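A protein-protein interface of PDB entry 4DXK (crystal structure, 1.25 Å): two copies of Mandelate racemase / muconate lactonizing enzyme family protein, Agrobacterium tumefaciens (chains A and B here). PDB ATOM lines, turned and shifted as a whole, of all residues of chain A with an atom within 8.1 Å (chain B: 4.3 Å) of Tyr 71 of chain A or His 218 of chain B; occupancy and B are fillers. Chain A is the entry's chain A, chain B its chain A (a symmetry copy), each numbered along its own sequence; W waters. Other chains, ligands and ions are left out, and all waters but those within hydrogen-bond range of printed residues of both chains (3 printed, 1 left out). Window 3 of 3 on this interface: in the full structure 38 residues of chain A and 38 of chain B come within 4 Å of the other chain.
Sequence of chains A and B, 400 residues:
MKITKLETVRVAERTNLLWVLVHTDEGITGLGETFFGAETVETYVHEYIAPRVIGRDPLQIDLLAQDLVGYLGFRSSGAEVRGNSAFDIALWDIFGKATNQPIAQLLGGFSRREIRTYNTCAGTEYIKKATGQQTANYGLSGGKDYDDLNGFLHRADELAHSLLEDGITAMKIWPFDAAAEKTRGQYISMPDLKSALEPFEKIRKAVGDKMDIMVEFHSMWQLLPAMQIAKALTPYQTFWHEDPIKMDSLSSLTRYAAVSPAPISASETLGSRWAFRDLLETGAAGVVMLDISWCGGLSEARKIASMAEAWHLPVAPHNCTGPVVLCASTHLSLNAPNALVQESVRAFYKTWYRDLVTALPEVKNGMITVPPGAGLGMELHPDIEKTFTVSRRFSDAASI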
ATOM      1  N   TYR A  48       2.539   0.230 -10.881  1.00  0.00           N
ATOM      2  CA  TYR A  48       3.510  -0.503 -11.695  1.00  0.00           C
ATOM      3  C   TYR A  48       4.844   0.226 -11.870  1.00  0.00           C
ATOM      4  O   TYR A  48       5.908  -0.357 -11.654  1.00  0.00           O
ATOM      5  CB  TYR A  48       2.907  -0.807 -13.073  1.00  0.00           C
ATOM      6  CG  TYR A  48       3.705  -1.815 -13.870  1.00  0.00           C
ATOM      7  CD1 TYR A  48       4.746  -1.424 -14.708  1.00  0.00           C
ATOM      8  CD2 TYR A  48       3.418  -3.169 -13.769  1.00  0.00           C
ATOM      9  CE1 TYR A  48       5.476  -2.354 -15.424  1.00  0.00           C
ATOM     10  CE2 TYR A  48       4.138  -4.108 -14.478  1.00  0.00           C
ATOM     11  CZ  TYR A  48       5.160  -3.696 -15.305  1.00  0.00           C
ATOM     12  OH  TYR A  48       5.868  -4.651 -16.000  1.00  0.00           O
ATOM     13  N   ARG A  52       9.155   0.017  -9.619  1.00  0.00           N
ATOM     14  CA  ARG A  52      10.253  -0.340 -10.503  1.00  0.00           C
ATOM     15  C   ARG A  52      11.281   0.767 -10.705  1.00  0.00           C
ATOM     16  O   ARG A  52      12.388   0.500 -11.176  1.00  0.00           O
ATOM     17  CB  ARG A  52       9.715  -0.775 -11.862  1.00  0.00           C
ATOM     18  CG  ARG A  52       9.051  -2.127 -11.806  1.00  0.00           C
ATOM     19  CD  ARG A  52       8.290  -2.451 -13.077  1.00  0.00           C
ATOM     20  NE  ARG A  52       7.771  -3.816 -13.036  1.00  0.00           N
ATOM     21  CZ  ARG A  52       6.715  -4.195 -12.328  1.00  0.00           C
ATOM     22  NH1 ARG A  52       6.037  -3.315 -11.604  1.00  0.00           N
ATOM     23  NH2 ARG A  52       6.324  -5.466 -12.348  1.00  0.00           N
ATOM     24  N   ASP A  67      12.878  -1.620 -19.283  1.00  0.00           N
ATOM     25  CA  ASP A  67      12.436  -2.202 -18.019  1.00  0.00           C
ATOM     26  C   ASP A  67      10.938  -2.034 -17.759  1.00  0.00           C
ATOM     27  O   ASP A  67      10.378  -2.745 -16.915  1.00  0.00           O
ATOM     28  CB  ASP A  67      13.235  -1.626 -16.841  1.00  0.00           C
ATOM     29  CG  ASP A  67      14.663  -2.141 -16.784  1.00  0.00           C
ATOM     30  OD1 ASP A  67      14.957  -3.151 -17.446  1.00  0.00           O
ATOM     31  OD2 ASP A  67      15.478  -1.537 -16.053  1.00  0.00           O
ATOM     32  N   LEU A  68      10.291  -1.098 -18.455  1.00  0.00           N
ATOM     33  CA  LEU A  68       8.859  -0.861 -18.255  1.00  0.00           C
ATOM     34  C   LEU A  68       7.972  -1.542 -19.298  1.00  0.00           C
ATOM     35  O   LEU A  68       6.749  -1.489 -19.185  1.00  0.00           O
ATOM     36  CB  LEU A  68       8.553   0.640 -18.174  1.00  0.00           C
ATOM     37  CG  LEU A  68       9.155   1.358 -16.962  1.00  0.00           C
ATOM     38  CD1 LEU A  68       8.791   2.832 -17.008  1.00  0.00           C
ATOM     39  CD2 LEU A  68       8.682   0.728 -15.652  1.00  0.00           C
ATOM     40  N   VAL A  69       8.565  -2.163 -20.315  1.00  0.00           N
ATOM     41  CA  VAL A  69       7.762  -2.911 -21.281  1.00  0.00           C
ATOM     42  C   VAL A  69       7.033  -4.044 -20.560  1.00  0.00           C
ATOM     43  O   VAL A  69       7.643  -4.824 -19.836  1.00  0.00           O
ATOM     44  CB  VAL A  69       8.615  -3.479 -22.422  1.00  0.00           C
ATOM     45  CG1 VAL A  69       7.772  -4.377 -23.311  1.00  0.00           C
ATOM     46  CG2 VAL A  69       9.253  -2.350 -23.252  1.00  0.00           C
ATOM     47  N   GLY A  70       5.723  -4.125 -20.747  1.00  0.00           N
ATOM     48  CA  GLY A  70       4.928  -5.104 -20.031  1.00  0.00           C
ATOM     49  C   GLY A  70       4.912  -6.470 -20.677  1.00  0.00           C
ATOM     50  O   GLY A  70       5.071  -6.605 -21.887  1.00  0.00           O
ATOM     51  N   TYR A  71       4.721  -7.497 -19.862  1.00  0.00           N
ATOM     52  CA  TYR A  71       4.424  -8.827 -20.362  1.00  0.00           C
ATOM     53  C   TYR A  71       3.129  -8.797 -21.176  1.00  0.00           C
ATOM     54  O   TYR A  71       2.993  -9.490 -22.187  1.00  0.00           O
ATOM     55  CB  TYR A  71       4.297  -9.792 -19.181  1.00  0.00           C
ATOM     56  CG  TYR A  71       4.016 -11.204 -19.595  1.00  0.00           C
ATOM     57  CD1 TYR A  71       4.991 -11.967 -20.227  1.00  0.00           C
ATOM     58  CD2 TYR A  71       2.781 -11.783 -19.350  1.00  0.00           C
ATOM     59  CE1 TYR A  71       4.738 -13.268 -20.603  1.00  0.00           C
ATOM     60  CE2 TYR A  71       2.517 -13.092 -19.724  1.00  0.00           C
ATOM     61  CZ  TYR A  71       3.502 -13.820 -20.357  1.00  0.00           C
ATOM     62  OH  TYR A  71       3.260 -15.122 -20.731  1.00  0.00           O
ATOM     63  N   LEU A  72       2.192  -7.975 -20.716  1.00  0.00           N
ATOM     64  CA  LEU A  72       0.939  -7.712 -21.424  1.00  0.00           C
ATOM     65  C   LEU A  72       0.843  -6.238 -21.778  1.00  0.00           C
ATOM     66  O   LEU A  72       1.484  -5.407 -21.141  1.00  0.00           O
ATOM     67  CB  LEU A  72      -0.259  -8.072 -20.544  1.00  0.00           C
ATOM     68  CG  LEU A  72      -0.335  -9.508 -20.042  1.00  0.00           C
ATOM     69  CD1 LEU A  72      -1.615  -9.706 -19.238  1.00  0.00           C
ATOM     70  CD2 LEU A  72      -0.279 -10.507 -21.181  1.00  0.00           C
ATOM     71  N   GLY A  73       0.053  -5.906 -22.795  1.00  0.00           N
ATOM     72  CA  GLY A  73      -0.242  -4.513 -23.095  1.00  0.00           C
ATOM     73  C   GLY A  73       0.812  -3.778 -23.900  1.00  0.00           C
ATOM     74  O   GLY A  73       0.698  -2.569 -24.116  1.00  0.00           O
ATOM     75  N   PHE A  74       1.819  -4.501 -24.368  1.00  0.00           N
ATOM     76  CA  PHE A  74       2.891  -3.954 -25.191  1.00  0.00           C
ATOM     77  C   PHE A  74       2.390  -3.751 -26.636  1.00  0.00           C
ATOM     78  O   PHE A  74       1.313  -4.219 -27.006  1.00  0.00           O
ATOM     79  CB  PHE A  74       4.081  -4.926 -25.149  1.00  0.00           C
ATOM     80  CG  PHE A  74       3.734  -6.284 -25.648  1.00  0.00           C
ATOM     81  CD1 PHE A  74       3.812  -6.588 -27.000  1.00  0.00           C
ATOM     82  CD2 PHE A  74       3.259  -7.258 -24.775  1.00  0.00           C
ATOM     83  CE1 PHE A  74       3.447  -7.833 -27.477  1.00  0.00           C
ATOM     84  CE2 PHE A  74       2.897  -8.503 -25.249  1.00  0.00           C
ATOM     85  CZ  PHE A  74       2.983  -8.797 -26.595  1.00  0.00           C
ATOM     86  N   GLU A  80      -1.009   1.240 -19.909  1.00  0.00           N
ATOM     87  CA  GLU A  80       0.361   0.996 -19.470  1.00  0.00           C
ATOM     88  C   GLU A  80       1.350   1.772 -20.344  1.00  0.00           C
ATOM     89  O   GLU A  80       2.270   2.430 -19.845  1.00  0.00           O
ATOM     90  CB  GLU A  80       0.693  -0.503 -19.509  1.00  0.00           C
ATOM     91  CG  GLU A  80      -0.133  -1.378 -18.563  1.00  0.00           C
ATOM     92  CD  GLU A  80      -1.374  -2.008 -19.172  1.00  0.00           C
ATOM     93  OE1 GLU A  80      -1.921  -1.513 -20.178  1.00  0.00           O
ATOM     94  OE2 GLU A  80      -1.811  -3.029 -18.609  1.00  0.00           O
ATOM     95  N   TRP B 174       9.314 -24.380 -17.925  1.00  0.00           N
ATOM     96  CA  TRP B 174      10.010 -23.205 -18.450  1.00  0.00           C
ATOM     97  C   TRP B 174      11.438 -23.096 -17.910  1.00  0.00           C
ATOM     98  O   TRP B 174      11.769 -22.150 -17.191  1.00  0.00           O
ATOM     99  CB  TRP B 174       9.220 -21.910 -18.192  1.00  0.00           C
ATOM    100  CG  TRP B 174       8.634 -21.740 -16.816  1.00  0.00           C
ATOM    101  CD1 TRP B 174       9.204 -21.107 -15.748  1.00  0.00           C
ATOM    102  CD2 TRP B 174       7.335 -22.159 -16.386  1.00  0.00           C
ATOM    103  NE1 TRP B 174       8.348 -21.130 -14.673  1.00  0.00           N
ATOM    104  CE2 TRP B 174       7.193 -21.770 -15.039  1.00  0.00           C
ATOM    105  CE3 TRP B 174       6.284 -22.838 -17.005  1.00  0.00           C
ATOM    106  CZ2 TRP B 174       6.042 -22.041 -14.300  1.00  0.00           C
ATOM    107  CZ3 TRP B 174       5.140 -23.101 -16.275  1.00  0.00           C
ATOM    108  CH2 TRP B 174       5.029 -22.706 -14.937  1.00  0.00           C
ATOM    109  N   ASP B 177      14.040 -19.768 -18.512  1.00  0.00           N
ATOM    110  CA  ASP B 177      13.760 -18.408 -18.056  1.00  0.00           C
ATOM    111  C   ASP B 177      14.930 -17.805 -17.274  1.00  0.00           C
ATOM    112  O   ASP B 177      15.223 -16.620 -17.400  1.00  0.00           O
ATOM    113  CB  ASP B 177      12.496 -18.352 -17.198  1.00  0.00           C
ATOM    114  CG  ASP B 177      11.213 -18.500 -18.006  1.00  0.00           C
ATOM    115  OD1 ASP B 177      11.239 -18.981 -19.156  1.00  0.00           O
ATOM    116  OD2 ASP B 177      10.151 -18.147 -17.452  1.00  0.00           O
ATOM    117  N   GLU B 216       7.432 -23.602 -22.264  1.00  0.00           N
ATOM    118  CA  GLU B 216       7.049 -22.215 -22.121  1.00  0.00           C
ATOM    119  C   GLU B 216       8.312 -21.359 -22.128  1.00  0.00           C
ATOM    120  O   GLU B 216       9.265 -21.682 -21.417  1.00  0.00           O
ATOM    121  CB  GLU B 216       6.364 -22.063 -20.766  1.00  0.00           C
ATOM    122  CG  GLU B 216       6.226 -20.656 -20.321  1.00  0.00           C
ATOM    123  CD  GLU B 216       5.151 -19.975 -21.096  1.00  0.00           C
ATOM    124  OE1 GLU B 216       5.463 -19.323 -22.116  1.00  0.00           O
ATOM    125  OE2 GLU B 216       3.982 -20.142 -20.698  1.00  0.00           O
ATOM    126  N   PHE B 217       8.320 -20.277 -22.905  1.00  0.00           N
ATOM    127  CA  PHE B 217       9.453 -19.347 -22.938  1.00  0.00           C
ATOM    128  C   PHE B 217       9.129 -17.950 -22.427  1.00  0.00           C
ATOM    129  O   PHE B 217      10.023 -17.114 -22.300  1.00  0.00           O
ATOM    130  CB  PHE B 217      10.012 -19.233 -24.356  1.00  0.00           C
ATOM    131  CG  PHE B 217      10.625 -20.500 -24.871  1.00  0.00           C
ATOM    132  CD1 PHE B 217      11.898 -20.884 -24.462  1.00  0.00           C
ATOM    133  CD2 PHE B 217       9.934 -21.318 -25.762  1.00  0.00           C
ATOM    134  CE1 PHE B 217      12.476 -22.041 -24.948  1.00  0.00           C
ATOM    135  CE2 PHE B 217      10.512 -22.484 -26.243  1.00  0.00           C
ATOM    136  CZ  PHE B 217      11.788 -22.840 -25.840  1.00  0.00           C
ATOM    137  N   HIS B 218       7.849 -17.689 -22.185  1.00  0.00           N
ATOM    138  CA  HIS B 218       7.399 -16.408 -21.633  1.00  0.00           C
ATOM    139  C   HIS B 218       7.873 -15.190 -22.429  1.00  0.00           C
ATOM    140  O   HIS B 218       8.069 -14.116 -21.867  1.00  0.00           O
ATOM    141  CB  HIS B 218       7.829 -16.282 -20.170  1.00  0.00           C
ATOM    142  CG  HIS B 218       7.075 -17.186 -19.245  1.00  0.00           C
ATOM    143  ND1 HIS B 218       7.701 -18.011 -18.337  1.00  0.00           N
ATOM    144  CD2 HIS B 218       5.747 -17.388 -19.088  1.00  0.00           C
ATOM    145  CE1 HIS B 218       6.788 -18.677 -17.648  1.00  0.00           C
ATOM    146  NE2 HIS B 218       5.594 -18.317 -18.086  1.00  0.00           N
ATOM    147  N   SER B 219       8.043 -15.358 -23.738  1.00  0.00           N
ATOM    148  CA  SER B 219       8.450 -14.269 -24.637  1.00  0.00           C
ATOM    149  C   SER B 219       9.759 -13.598 -24.242  1.00  0.00           C
ATOM    150  O   SER B 219       9.962 -12.419 -24.528  1.00  0.00           O
ATOM    151  CB  SER B 219       7.346 -13.214 -24.777  1.00  0.00           C
ATOM    152  OG  SER B 219       6.276 -13.763 -25.532  1.00  0.00           O
ATOM    153  N   MET B 220      10.654 -14.355 -23.616  1.00  0.00           N
ATOM    154  CA  MET B 220      11.852 -13.755 -23.035  1.00  0.00           C
ATOM    155  C   MET B 220      13.078 -13.700 -23.946  1.00  0.00           C
ATOM    156  O   MET B 220      14.085 -13.098 -23.579  1.00  0.00           O
ATOM    157  CB  MET B 220      12.201 -14.451 -21.721  1.00  0.00           C
ATOM    158  CG  MET B 220      11.050 -14.429 -20.724  1.00  0.00           C
ATOM    159  SD  MET B 220      11.444 -15.179 -19.139  1.00  0.00           S
ATOM    160  CE  MET B 220      12.730 -14.077 -18.574  1.00  0.00           C
ATOM    161  N   GLU B 242       6.029 -22.419 -26.689  1.00  0.00           N
ATOM    162  CA  GLU B 242       5.086 -21.344 -26.405  1.00  0.00           C
ATOM    163  C   GLU B 242       5.802 -20.020 -26.198  1.00  0.00           C
ATOM    164  O   GLU B 242       6.756 -19.925 -25.412  1.00  0.00           O
ATOM    165  CB  GLU B 242       4.274 -21.710 -25.165  1.00  0.00           C
ATOM    166  CG  GLU B 242       3.192 -20.703 -24.782  1.00  0.00           C
ATOM    167  CD  GLU B 242       2.322 -21.210 -23.647  1.00  0.00           C
ATOM    168  OE1 GLU B 242       2.280 -22.435 -23.411  1.00  0.00           O
ATOM    169  OE2 GLU B 242       1.685 -20.382 -22.957  1.00  0.00           O
ATOM    170  N   ASP B 243       5.331 -18.996 -26.902  1.00  0.00           N
ATOM    171  CA  ASP B 243       5.870 -17.643 -26.791  1.00  0.00           C
ATOM    172  C   ASP B 243       7.402 -17.625 -26.832  1.00  0.00           C
ATOM    173  O   ASP B 243       8.051 -17.093 -25.934  1.00  0.00           O
ATOM    174  CB  ASP B 243       5.309 -16.960 -25.541  1.00  0.00           C
ATOM    175  CG  ASP B 243       3.837 -16.647 -25.674  1.00  0.00           C
ATOM    176  OD1 ASP B 243       3.400 -16.430 -26.811  1.00  0.00           O
ATOM    177  OD2 ASP B 243       3.120 -16.618 -24.657  1.00  0.00           O
ATOM    178  N   LYS B 246       8.977 -12.340 -28.287  1.00  0.00           N
ATOM    179  CA  LYS B 246       7.936 -11.352 -28.022  1.00  0.00           C
ATOM    180  C   LYS B 246       6.970 -11.329 -29.193  1.00  0.00           C
ATOM    181  O   LYS B 246       7.383 -11.374 -30.350  1.00  0.00           O
ATOM    182  CB  LYS B 246       8.562  -9.967 -27.851  1.00  0.00           C
ATOM    183  CG  LYS B 246       7.644  -8.945 -27.206  1.00  0.00           C
ATOM    184  CD  LYS B 246       7.549  -9.141 -25.714  1.00  0.00           C
ATOM    185  CE  LYS B 246       6.856  -7.955 -25.047  1.00  0.00           C
ATOM    186  NZ  LYS B 246       6.670  -8.248 -23.619  1.00  0.00           N
ATOM    187  N   GLU B 268      -1.139 -16.238 -25.439  1.00  0.00           N
ATOM    188  CA  GLU B 268      -1.935 -15.625 -24.380  1.00  0.00           C
ATOM    189  C   GLU B 268      -1.731 -14.107 -24.316  1.00  0.00           C
ATOM    190  O   GLU B 268      -2.564 -13.388 -23.760  1.00  0.00           O
ATOM    191  CB  GLU B 268      -1.569 -16.255 -23.032  1.00  0.00           C
ATOM    192  CG  GLU B 268      -0.146 -15.915 -22.572  1.00  0.00           C
ATOM    193  CD  GLU B 268       0.349 -16.735 -21.394  1.00  0.00           C
ATOM    194  OE1 GLU B 268       0.108 -17.954 -21.375  1.00  0.00           O
ATOM    195  OE2 GLU B 268       0.994 -16.157 -20.487  1.00  0.00           O
ATOM    196  N   THR B 269      -0.623 -13.619 -24.868  1.00  0.00           N
ATOM    197  CA  THR B 269      -0.330 -12.181 -24.809  1.00  0.00           C
ATOM    198  C   THR B 269      -1.003 -11.350 -25.898  1.00  0.00           C
ATOM    199  O   THR B 269      -0.939 -10.123 -25.841  1.00  0.00           O
ATOM    200  CB  THR B 269       1.196 -11.875 -24.837  1.00  0.00           C
ATOM    201  OG1 THR B 269       1.735 -12.141 -26.142  1.00  0.00           O
ATOM    202  CG2 THR B 269       1.940 -12.701 -23.800  1.00  0.00           C
HETATM  203  O   HOH W   1       5.138 -10.613 -23.518  1.00  0.00           O
HETATM  204  O   HOH W   2       4.676 -15.128 -23.064  1.00  0.00           O
HETATM  205  O   HOH W   3       2.487 -17.782 -19.156  1.00  0.00           O
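The backbone carbonyl oxygen of Gly 70 of chain A is in hydrogen-bond range of the side-chain amino group of Lys 246 of chain B (2.9 Å).
The side-chain hydroxyl of Tyr 71 of chain A is in hydrogen-bond range of the side-chain carboxylate of Glu 268 of chain B, 2.5 Å away.
The side-chain carboxylate of Asp 177 of chain B lies within hydrogen-bond range of a ring nitrogen (ND1) of His 218 of chain B (2.6 Å).
The side-chain carboxylate (OE1) of Glu 216 of chain B is in hydrogen-bond range of the backbone NH (N) of His 218 of chain B (2.9 Å).
Among the printed residues, merely in contact across the chains: Phe 74 of chain A with Lys 246 of chain B (3.6 Å), Phe 74 of chain A with Thr 269 of chain B (3.6 Å), Tyr 71 of chain A with His 218 of chain B (3.7 Å), Tyr 71 of chain A with Thr 269 of chain B (3.7 Å), Leu 72 of chain A with Thr 269 of chain B (3.996 Å) and Tyr 71 of chain A with Lys 246 of chain B (3.998 Å).
Of the printed residues of chain B, Gly 70 of chain A touches Lys 246.
Of the printed residues of chain B, Tyr 71 of chain A touches His 218, Lys 246, Glu 268 and Thr 269.
Of the printed residues of chain B, Leu 72 of chain A touches Thr 269.
Gly 73 of chain A touches none of the printed residues of chain B.
His 218 of chain B touches just one residue of chain A: Tyr 71 (3.7 Å).
No residue of chain A comes within 4 Å of Ser 219 of chain B.
Of the printed residues of chain A, Lys 246 of chain B touches Gly 70 (2.9 Å), Tyr 71 (3.998 Å) and Phe 74 (3.6 Å).
Of the printed residues of chain A, Glu 268 of chain B touches Tyr 71 (2.5 Å).
Printed residues of chain A within 4 Å of Thr 269 of chain B: Tyr 71, Leu 72 and Phe 74.
The nearest printed residue of chain B that does not touch Tyr 71 of chain A is Asp 243 of chain B (4.2 Å).
The nearest printed residue of chain A that does not touch Thr 269 of chain B is Gly 73 of chain A (5.3 Å).
Hydrophobic or aromatic side chains of chain A that line the printed part of chain B: Tyr 71, Leu 72 and Phe 74.
Of the 12 printed residues of chain B, 4 touch a printed residue of chain A.
Printed residues of chain B that touch a printed residue of chain A: His 218, Lys 246, Glu 268 and Thr 269.
Among the printed residues, 8 pairs touch across the chains.
Among the printed residues, no Asp or Glu carboxylate lies within 4 Å of a Lys or Arg side-chain nitrogen of the other chain.
No position is printed for both chains.
Water W3 lies within hydrogen-bond range of the side-chain carboxylate of Glu 268 of chain B, the side-chain hydroxyl of Tyr 71 of chain A, the side-chain carboxylate of Glu 216 of chain B and a ring nitrogen (NE2) of His 218 of chain B.
Water W2 lies within hydrogen-bond range of the side-chain carboxylate of Asp 243 of chain B (2.7 Å), the side-chain hydroxyl of Tyr 71 of chain A (2.7 Å) and the side-chain hydroxyl of Ser 219 of chain B (3.2 Å).
Water W1 bridges O of Tyr 71 of chain A (2.8 Å) and NZ of Lys 246 of chain B (2.8 Å).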
